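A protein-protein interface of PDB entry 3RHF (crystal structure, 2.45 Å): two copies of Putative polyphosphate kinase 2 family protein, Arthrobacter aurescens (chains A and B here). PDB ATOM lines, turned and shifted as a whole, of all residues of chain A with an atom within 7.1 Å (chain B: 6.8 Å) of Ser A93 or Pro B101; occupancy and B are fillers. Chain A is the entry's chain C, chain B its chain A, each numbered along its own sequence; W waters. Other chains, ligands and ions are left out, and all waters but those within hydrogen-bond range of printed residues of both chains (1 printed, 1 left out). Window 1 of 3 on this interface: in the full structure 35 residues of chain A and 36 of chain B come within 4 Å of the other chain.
Among the printed residues, pairs that only touch across the chains: Ser A93 with Pro B101 (3.6 Å), Ser A93 with Met B99 (3.7 Å), Leu A106 with Pro B101 (3.8 Å), Ser A93 with Asp B100 (3.8 Å) and Gly A97 with Gly B97 (3.996 Å).
Of the 12 printed residues of chain B, 4 touch a printed residue of chain A.
Printed residues of chain B that touch a printed residue of chain A: Gly B97, Met B99, Asp B100 and Pro B101.
Hydrophobic or aromatic side chains of chain B that line the printed part of chain A: Pro B101.
Printed residues of chain A that touch a printed residue of chain B: Ser A93, Gly A97 and Leu A106.
Gly B97 touches its own counterpart, Gly A97.
Water W1 lies within hydrogen-bond range of the side-chain amide nitrogen of Gln B102, the side-chain carboxylate of Asp B100 and the backbone carbonyl oxygen of Gly A89.
Gly A90 touches none of the printed residues of chain B.
Of the printed residues of chain B, Gly A97 touches Gly B97.
Of the printed residues of chain B, Leu A106 touches Pro B101.
Of the printed residues of chain A, Gly B97 touches Gly A97.
Of the printed residues of chain A, Met B99 touches Ser A93 (3.7 Å).
Of chain A, only Ser A93 (3.6 Å) and Leu A106 (3.8 Å) come within 4 Å of Pro B101.
Gly B103 touches none of the printed residues of chain A.
The nearest residue of chain B that does not touch Ser A93 is Gly B97 (5.5 Å).
The nearest residue of chain A that does not touch Pro B101 is Val A96 (4.3 Å).
OE1 of Gln B61 sits at hydrogen-bond distance from N of Asp B100 (2.9 Å).
OD2 of Asp B100 sits at hydrogen-bond distance from N of Gln B102 (3.0 Å).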
ATOM      1  N   GLY A  87      -7.740  13.404  10.572  1.00  0.00           N
ATOM      2  CA  GLY A  87      -8.299  12.644  11.693  1.00  0.00           C
ATOM      3  C   GLY A  87      -9.797  12.847  11.987  1.00  0.00           C
ATOM      4  O   GLY A  87     -10.340  12.254  12.921  1.00  0.00           O
ATOM      5  N   LYS A  88     -10.448  13.691  11.210  1.00  0.00           N
ATOM      6  CA  LYS A  88     -11.843  14.131  11.455  1.00  0.00           C
ATOM      7  C   LYS A  88     -12.849  12.952  11.572  1.00  0.00           C
ATOM      8  O   LYS A  88     -13.563  12.823  12.589  1.00  0.00           O
ATOM      9  CB  LYS A  88     -12.199  15.113  10.331  1.00  0.00           C
ATOM     10  CG  LYS A  88     -13.576  15.771  10.305  1.00  0.00           C
ATOM     11  CD  LYS A  88     -13.760  16.618   8.921  1.00  0.00           C
ATOM     12  CE  LYS A  88     -13.591  15.746   7.605  1.00  0.00           C
ATOM     13  NZ  LYS A  88     -12.318  16.047   6.687  1.00  0.00           N
ATOM     14  N   GLY A  89     -12.851  12.045  10.592  1.00  0.00           N
ATOM     15  CA  GLY A  89     -13.683  10.859  10.662  1.00  0.00           C
ATOM     16  C   GLY A  89     -13.415  10.002  11.881  1.00  0.00           C
ATOM     17  O   GLY A  89     -14.306   9.541  12.555  1.00  0.00           O
ATOM     18  N   GLY A  90     -12.158   9.773  12.161  1.00  0.00           N
ATOM     19  CA  GLY A  90     -11.761   9.058  13.352  1.00  0.00           C
ATOM     20  C   GLY A  90     -12.275   9.702  14.594  1.00  0.00           C
ATOM     21  O   GLY A  90     -12.859   9.015  15.409  1.00  0.00           O
ATOM     22  N   ILE A  91     -12.113  11.014  14.727  1.00  0.00           N
ATOM     23  CA  ILE A  91     -12.630  11.695  15.894  1.00  0.00           C
ATOM     24  C   ILE A  91     -14.158  11.657  15.979  1.00  0.00           C
ATOM     25  O   ILE A  91     -14.726  11.462  17.044  1.00  0.00           O
ATOM     26  CB  ILE A  91     -12.160  13.167  15.943  1.00  0.00           C
ATOM     27  CG1 ILE A  91     -10.661  13.219  16.264  1.00  0.00           C
ATOM     28  CG2 ILE A  91     -12.937  14.019  17.017  1.00  0.00           C
ATOM     29  CD1 ILE A  91     -10.233  14.632  16.536  1.00  0.00           C
ATOM     30  N   VAL A  92     -14.828  11.846  14.855  1.00  0.00           N
ATOM     31  CA  VAL A  92     -16.261  11.719  14.839  1.00  0.00           C
ATOM     32  C   VAL A  92     -16.674  10.300  15.272  1.00  0.00           C
ATOM     33  O   VAL A  92     -17.631  10.123  16.050  1.00  0.00           O
ATOM     34  CB  VAL A  92     -16.795  11.909  13.429  1.00  0.00           C
ATOM     35  CG1 VAL A  92     -18.146  11.275  13.322  1.00  0.00           C
ATOM     36  CG2 VAL A  92     -16.744  13.392  13.074  1.00  0.00           C
ATOM     37  N   SER A  93     -15.954   9.300  14.757  1.00  0.00           N
ATOM     38  CA  SER A  93     -16.261   7.939  15.104  1.00  0.00           C
ATOM     39  C   SER A  93     -16.193   7.784  16.626  1.00  0.00           C
ATOM     40  O   SER A  93     -17.085   7.229  17.232  1.00  0.00           O
ATOM     41  CB  SER A  93     -15.293   6.959  14.434  1.00  0.00           C
ATOM     42  OG  SER A  93     -15.706   5.629  14.666  1.00  0.00           O
ATOM     43  N   HIS A  94     -15.151   8.317  17.229  1.00  0.00           N
ATOM     44  CA  HIS A  94     -14.893   7.999  18.604  1.00  0.00           C
ATOM     45  C   HIS A  94     -15.858   8.726  19.532  1.00  0.00           C
ATOM     46  O   HIS A  94     -16.347   8.147  20.498  1.00  0.00           O
ATOM     47  CB  HIS A  94     -13.481   8.357  18.979  1.00  0.00           C
ATOM     48  CG  HIS A  94     -13.131   7.929  20.346  1.00  0.00           C
ATOM     49  ND1 HIS A  94     -13.268   8.760  21.435  1.00  0.00           N
ATOM     50  CD2 HIS A  94     -12.703   6.732  20.825  1.00  0.00           C
ATOM     51  CE1 HIS A  94     -12.925   8.097  22.529  1.00  0.00           C
ATOM     52  NE2 HIS A  94     -12.581   6.866  22.187  1.00  0.00           N
ATOM     53  N   VAL A  95     -16.100  10.001  19.252  1.00  0.00           N
ATOM     54  CA  VAL A  95     -17.033  10.800  20.007  1.00  0.00           C
ATOM     55  C   VAL A  95     -18.445  10.239  19.901  1.00  0.00           C
ATOM     56  O   VAL A  95     -19.136  10.013  20.891  1.00  0.00           O
ATOM     57  CB  VAL A  95     -16.961  12.277  19.542  1.00  0.00           C
ATOM     58  CG1 VAL A  95     -18.222  12.984  19.840  1.00  0.00           C
ATOM     59  CG2 VAL A  95     -15.826  12.975  20.226  1.00  0.00           C
ATOM     60  N   VAL A  96     -18.890   9.954  18.712  1.00  0.00           N
ATOM     61  CA  VAL A  96     -20.215   9.320  18.577  1.00  0.00           C
ATOM     62  C   VAL A  96     -20.303   7.956  19.277  1.00  0.00           C
ATOM     63  O   VAL A  96     -21.359   7.597  19.812  1.00  0.00           O
ATOM     64  CB  VAL A  96     -20.595   9.233  17.114  1.00  0.00           C
ATOM     65  CG1 VAL A  96     -21.791   8.348  16.865  1.00  0.00           C
ATOM     66  CG2 VAL A  96     -20.829  10.642  16.630  1.00  0.00           C
ATOM     67  N   GLY A  97     -19.209   7.208  19.303  1.00  0.00           N
ATOM     68  CA  GLY A  97     -19.226   5.873  19.904  1.00  0.00           C
ATOM     69  C   GLY A  97     -19.235   5.923  21.437  1.00  0.00           C
ATOM     70  O   GLY A  97     -19.466   4.931  22.094  1.00  0.00           O
ATOM     71  N   ALA A  98     -18.915   7.080  22.000  1.00  0.00           N
ATOM     72  CA  ALA A  98     -18.887   7.251  23.399  1.00  0.00           C
ATOM     73  C   ALA A  98     -20.329   7.514  23.829  1.00  0.00           C
ATOM     74  O   ALA A  98     -20.625   7.296  24.994  1.00  0.00           O
ATOM     75  CB  ALA A  98     -17.994   8.400  23.775  1.00  0.00           C
ATOM     76  N   MET A  99     -21.211   7.948  22.894  1.00  0.00           N
ATOM     77  CA  MET A  99     -22.591   8.297  23.194  1.00  0.00           C
ATOM     78  C   MET A  99     -23.590   7.201  22.794  1.00  0.00           C
ATOM     79  O   MET A  99     -23.198   6.241  22.180  1.00  0.00           O
ATOM     80  CB  MET A  99     -22.938   9.623  22.554  1.00  0.00           C
ATOM     81  CG  MET A  99     -22.098  10.755  23.083  1.00  0.00           C
ATOM     82  SD  MET A  99     -22.431  12.413  22.157  1.00  0.00           S
ATOM     83  CE  MET A  99     -22.048  13.605  23.600  1.00  0.00           C
ATOM     84  N   LEU A 106     -25.847  12.524  13.456  1.00  0.00           N
ATOM     85  CA  LEU A 106     -24.594  12.765  12.728  1.00  0.00           C
ATOM     86  C   LEU A 106     -24.910  12.984  11.252  1.00  0.00           C
ATOM     87  O   LEU A 106     -25.602  12.170  10.650  1.00  0.00           O
ATOM     88  CB  LEU A 106     -23.669  11.586  12.888  1.00  0.00           C
ATOM     89  CG  LEU A 106     -22.516  11.547  11.886  1.00  0.00           C
ATOM     90  CD1 LEU A 106     -21.479  12.671  12.113  1.00  0.00           C
ATOM     91  CD2 LEU A 106     -21.864  10.186  11.973  1.00  0.00           C
ATOM     92  N   GLN B  61     -16.230  -4.608   9.745  1.00  0.00           N
ATOM     93  CA  GLN B  61     -17.207  -3.710   9.201  1.00  0.00           C
ATOM     94  C   GLN B  61     -16.515  -2.775   8.217  1.00  0.00           C
ATOM     95  O   GLN B  61     -17.052  -2.441   7.192  1.00  0.00           O
ATOM     96  CB  GLN B  61     -17.924  -2.949  10.333  1.00  0.00           C
ATOM     97  CG  GLN B  61     -18.828  -1.820   9.914  1.00  0.00           C
ATOM     98  CD  GLN B  61     -18.100  -0.491   9.747  1.00  0.00           C
ATOM     99  OE1 GLN B  61     -17.454   0.007  10.679  1.00  0.00           O
ATOM    100  NE2 GLN B  61     -18.194   0.095   8.534  1.00  0.00           N
ATOM    101  N   VAL B  96     -23.123  -0.590  17.576  1.00  0.00           N
ATOM    102  CA  VAL B  96     -22.905   0.579  16.759  1.00  0.00           C
ATOM    103  C   VAL B  96     -21.647   1.332  17.130  1.00  0.00           C
ATOM    104  O   VAL B  96     -20.875   1.757  16.250  1.00  0.00           O
ATOM    105  CB  VAL B  96     -24.147   1.479  16.803  1.00  0.00           C
ATOM    106  CG1 VAL B  96     -23.815   2.837  16.344  1.00  0.00           C
ATOM    107  CG2 VAL B  96     -25.263   0.833  15.953  1.00  0.00           C
ATOM    108  N   GLY B  97     -21.380   1.439  18.411  1.00  0.00           N
ATOM    109  CA  GLY B  97     -20.199   2.139  18.864  1.00  0.00           C
ATOM    110  C   GLY B  97     -18.900   1.449  18.614  1.00  0.00           C
ATOM    111  O   GLY B  97     -17.854   2.042  18.748  1.00  0.00           O
ATOM    112  N   ALA B  98     -18.926   0.173  18.306  1.00  0.00           N
ATOM    113  CA  ALA B  98     -17.691  -0.531  17.953  1.00  0.00           C
ATOM    114  C   ALA B  98     -17.410  -0.251  16.500  1.00  0.00           C
ATOM    115  O   ALA B  98     -16.307  -0.517  16.050  1.00  0.00           O
ATOM    116  CB  ALA B  98     -17.812  -2.025  18.168  1.00  0.00           C
ATOM    117  N   MET B  99     -18.401   0.262  15.759  1.00  0.00           N
ATOM    118  CA  MET B  99     -18.281   0.450  14.303  1.00  0.00           C
ATOM    119  C   MET B  99     -18.032   1.911  13.917  1.00  0.00           C
ATOM    120  O   MET B  99     -18.137   2.805  14.748  1.00  0.00           O
ATOM    121  CB  MET B  99     -19.533  -0.076  13.628  1.00  0.00           C
ATOM    122  CG  MET B  99     -19.638  -1.554  13.758  1.00  0.00           C
ATOM    123  SD  MET B  99     -21.178  -2.315  12.857  1.00  0.00           S
ATOM    124  CE  MET B  99     -20.534  -4.130  12.943  1.00  0.00           C
ATOM    125  N   ASP B 100     -17.649   2.153  12.666  1.00  0.00           N
ATOM    126  CA  ASP B 100     -17.647   3.518  12.158  1.00  0.00           C
ATOM    127  C   ASP B 100     -19.073   3.865  11.759  1.00  0.00           C
ATOM    128  O   ASP B 100     -19.621   3.191  10.930  1.00  0.00           O
ATOM    129  CB  ASP B 100     -16.682   3.714  10.989  1.00  0.00           C
ATOM    130  CG  ASP B 100     -16.451   5.226  10.648  1.00  0.00           C
ATOM    131  OD1 ASP B 100     -15.252   5.645  10.589  1.00  0.00           O
ATOM    132  OD2 ASP B 100     -17.455   5.974  10.454  1.00  0.00           O
ATOM    133  N   PRO B 101     -19.652   4.928  12.355  1.00  0.00           N
ATOM    134  CA  PRO B 101     -21.049   5.319  12.119  1.00  0.00           C
ATOM    135  C   PRO B 101     -21.377   5.643  10.678  1.00  0.00           C
ATOM    136  O   PRO B 101     -22.513   5.501  10.271  1.00  0.00           O
ATOM    137  CB  PRO B 101     -21.237   6.574  12.987  1.00  0.00           C
ATOM    138  CG  PRO B 101     -19.859   7.091  13.259  1.00  0.00           C
ATOM    139  CD  PRO B 101     -18.954   5.898  13.226  1.00  0.00           C
ATOM    140  N   GLN B 102     -20.396   6.043   9.888  1.00  0.00           N
ATOM    141  CA  GLN B 102     -20.647   6.282   8.488  1.00  0.00           C
ATOM    142  C   GLN B 102     -20.830   4.987   7.736  1.00  0.00           C
ATOM    143  O   GLN B 102     -21.250   5.004   6.589  1.00  0.00           O
ATOM    144  CB  GLN B 102     -19.561   7.180   7.917  1.00  0.00           C
ATOM    145  CG  GLN B 102     -19.651   8.607   8.610  1.00  0.00           C
ATOM    146  CD  GLN B 102     -18.566   9.643   8.207  1.00  0.00           C
ATOM    147  OE1 GLN B 102     -18.228   9.795   7.025  1.00  0.00           O
ATOM    148  NE2 GLN B 102     -18.080  10.414   9.204  1.00  0.00           N
ATOM    149  N   GLY B 103     -20.640   3.859   8.423  1.00  0.00           N
ATOM    150  CA  GLY B 103     -20.817   2.500   7.839  1.00  0.00           C
ATOM    151  C   GLY B 103     -22.049   1.763   8.365  1.00  0.00           C
ATOM    152  O   GLY B 103     -22.270   0.611   8.016  1.00  0.00           O
ATOM    153  N   VAL B 104     -22.870   2.485   9.143  1.00  0.00           N
ATOM    154  CA  VAL B 104     -24.013   1.915   9.865  1.00  0.00           C
ATOM    155  C   VAL B 104     -25.274   2.678   9.638  1.00  0.00           C
ATOM    156  O   VAL B 104     -25.244   3.898   9.652  1.00  0.00           O
ATOM    157  CB  VAL B 104     -23.751   1.927  11.396  1.00  0.00           C
ATOM    158  CG1 VAL B 104     -24.948   1.440  12.166  1.00  0.00           C
ATOM    159  CG2 VAL B 104     -22.564   1.056  11.708  1.00  0.00           C
ATOM    160  N   GLN B 105     -26.378   1.975   9.425  1.00  0.00           N
ATOM    161  CA  GLN B 105     -27.736   2.620   9.263  1.00  0.00           C
ATOM    162  C   GLN B 105     -28.577   2.011  10.375  1.00  0.00           C
ATOM    163  O   GLN B 105     -28.978   0.854  10.298  1.00  0.00           O
ATOM    164  CB  GLN B 105     -28.406   2.441   7.851  1.00  0.00           C
ATOM    165  CG  GLN B 105     -27.373   2.510   6.680  1.00  0.00           C
ATOM    166  CD  GLN B 105     -27.899   2.578   5.206  1.00  0.00           C
ATOM    167  OE1 GLN B 105     -27.776   1.608   4.411  1.00  0.00           O
ATOM    168  NE2 GLN B 105     -28.375   3.738   4.828  1.00  0.00           N
ATOM    169  N   MET B 134     -23.143  -1.614   3.816  1.00  0.00           N
ATOM    170  CA  MET B 134     -23.558  -1.065   5.084  1.00  0.00           C
ATOM    171  C   MET B 134     -23.948  -2.151   6.072  1.00  0.00           C
ATOM    172  O   MET B 134     -24.301  -3.269   5.670  1.00  0.00           O
ATOM    173  CB  MET B 134     -24.710  -0.112   4.903  1.00  0.00           C
ATOM    174  CG  MET B 134     -24.467   1.051   3.919  1.00  0.00           C
ATOM    175  SD  MET B 134     -23.207   2.376   4.617  1.00  0.00           S
ATOM    176  CE  MET B 134     -24.265   3.259   6.002  1.00  0.00           C
HETATM  177  O   HOH W   1     -16.991   8.766  11.217  1.00  0.00           O
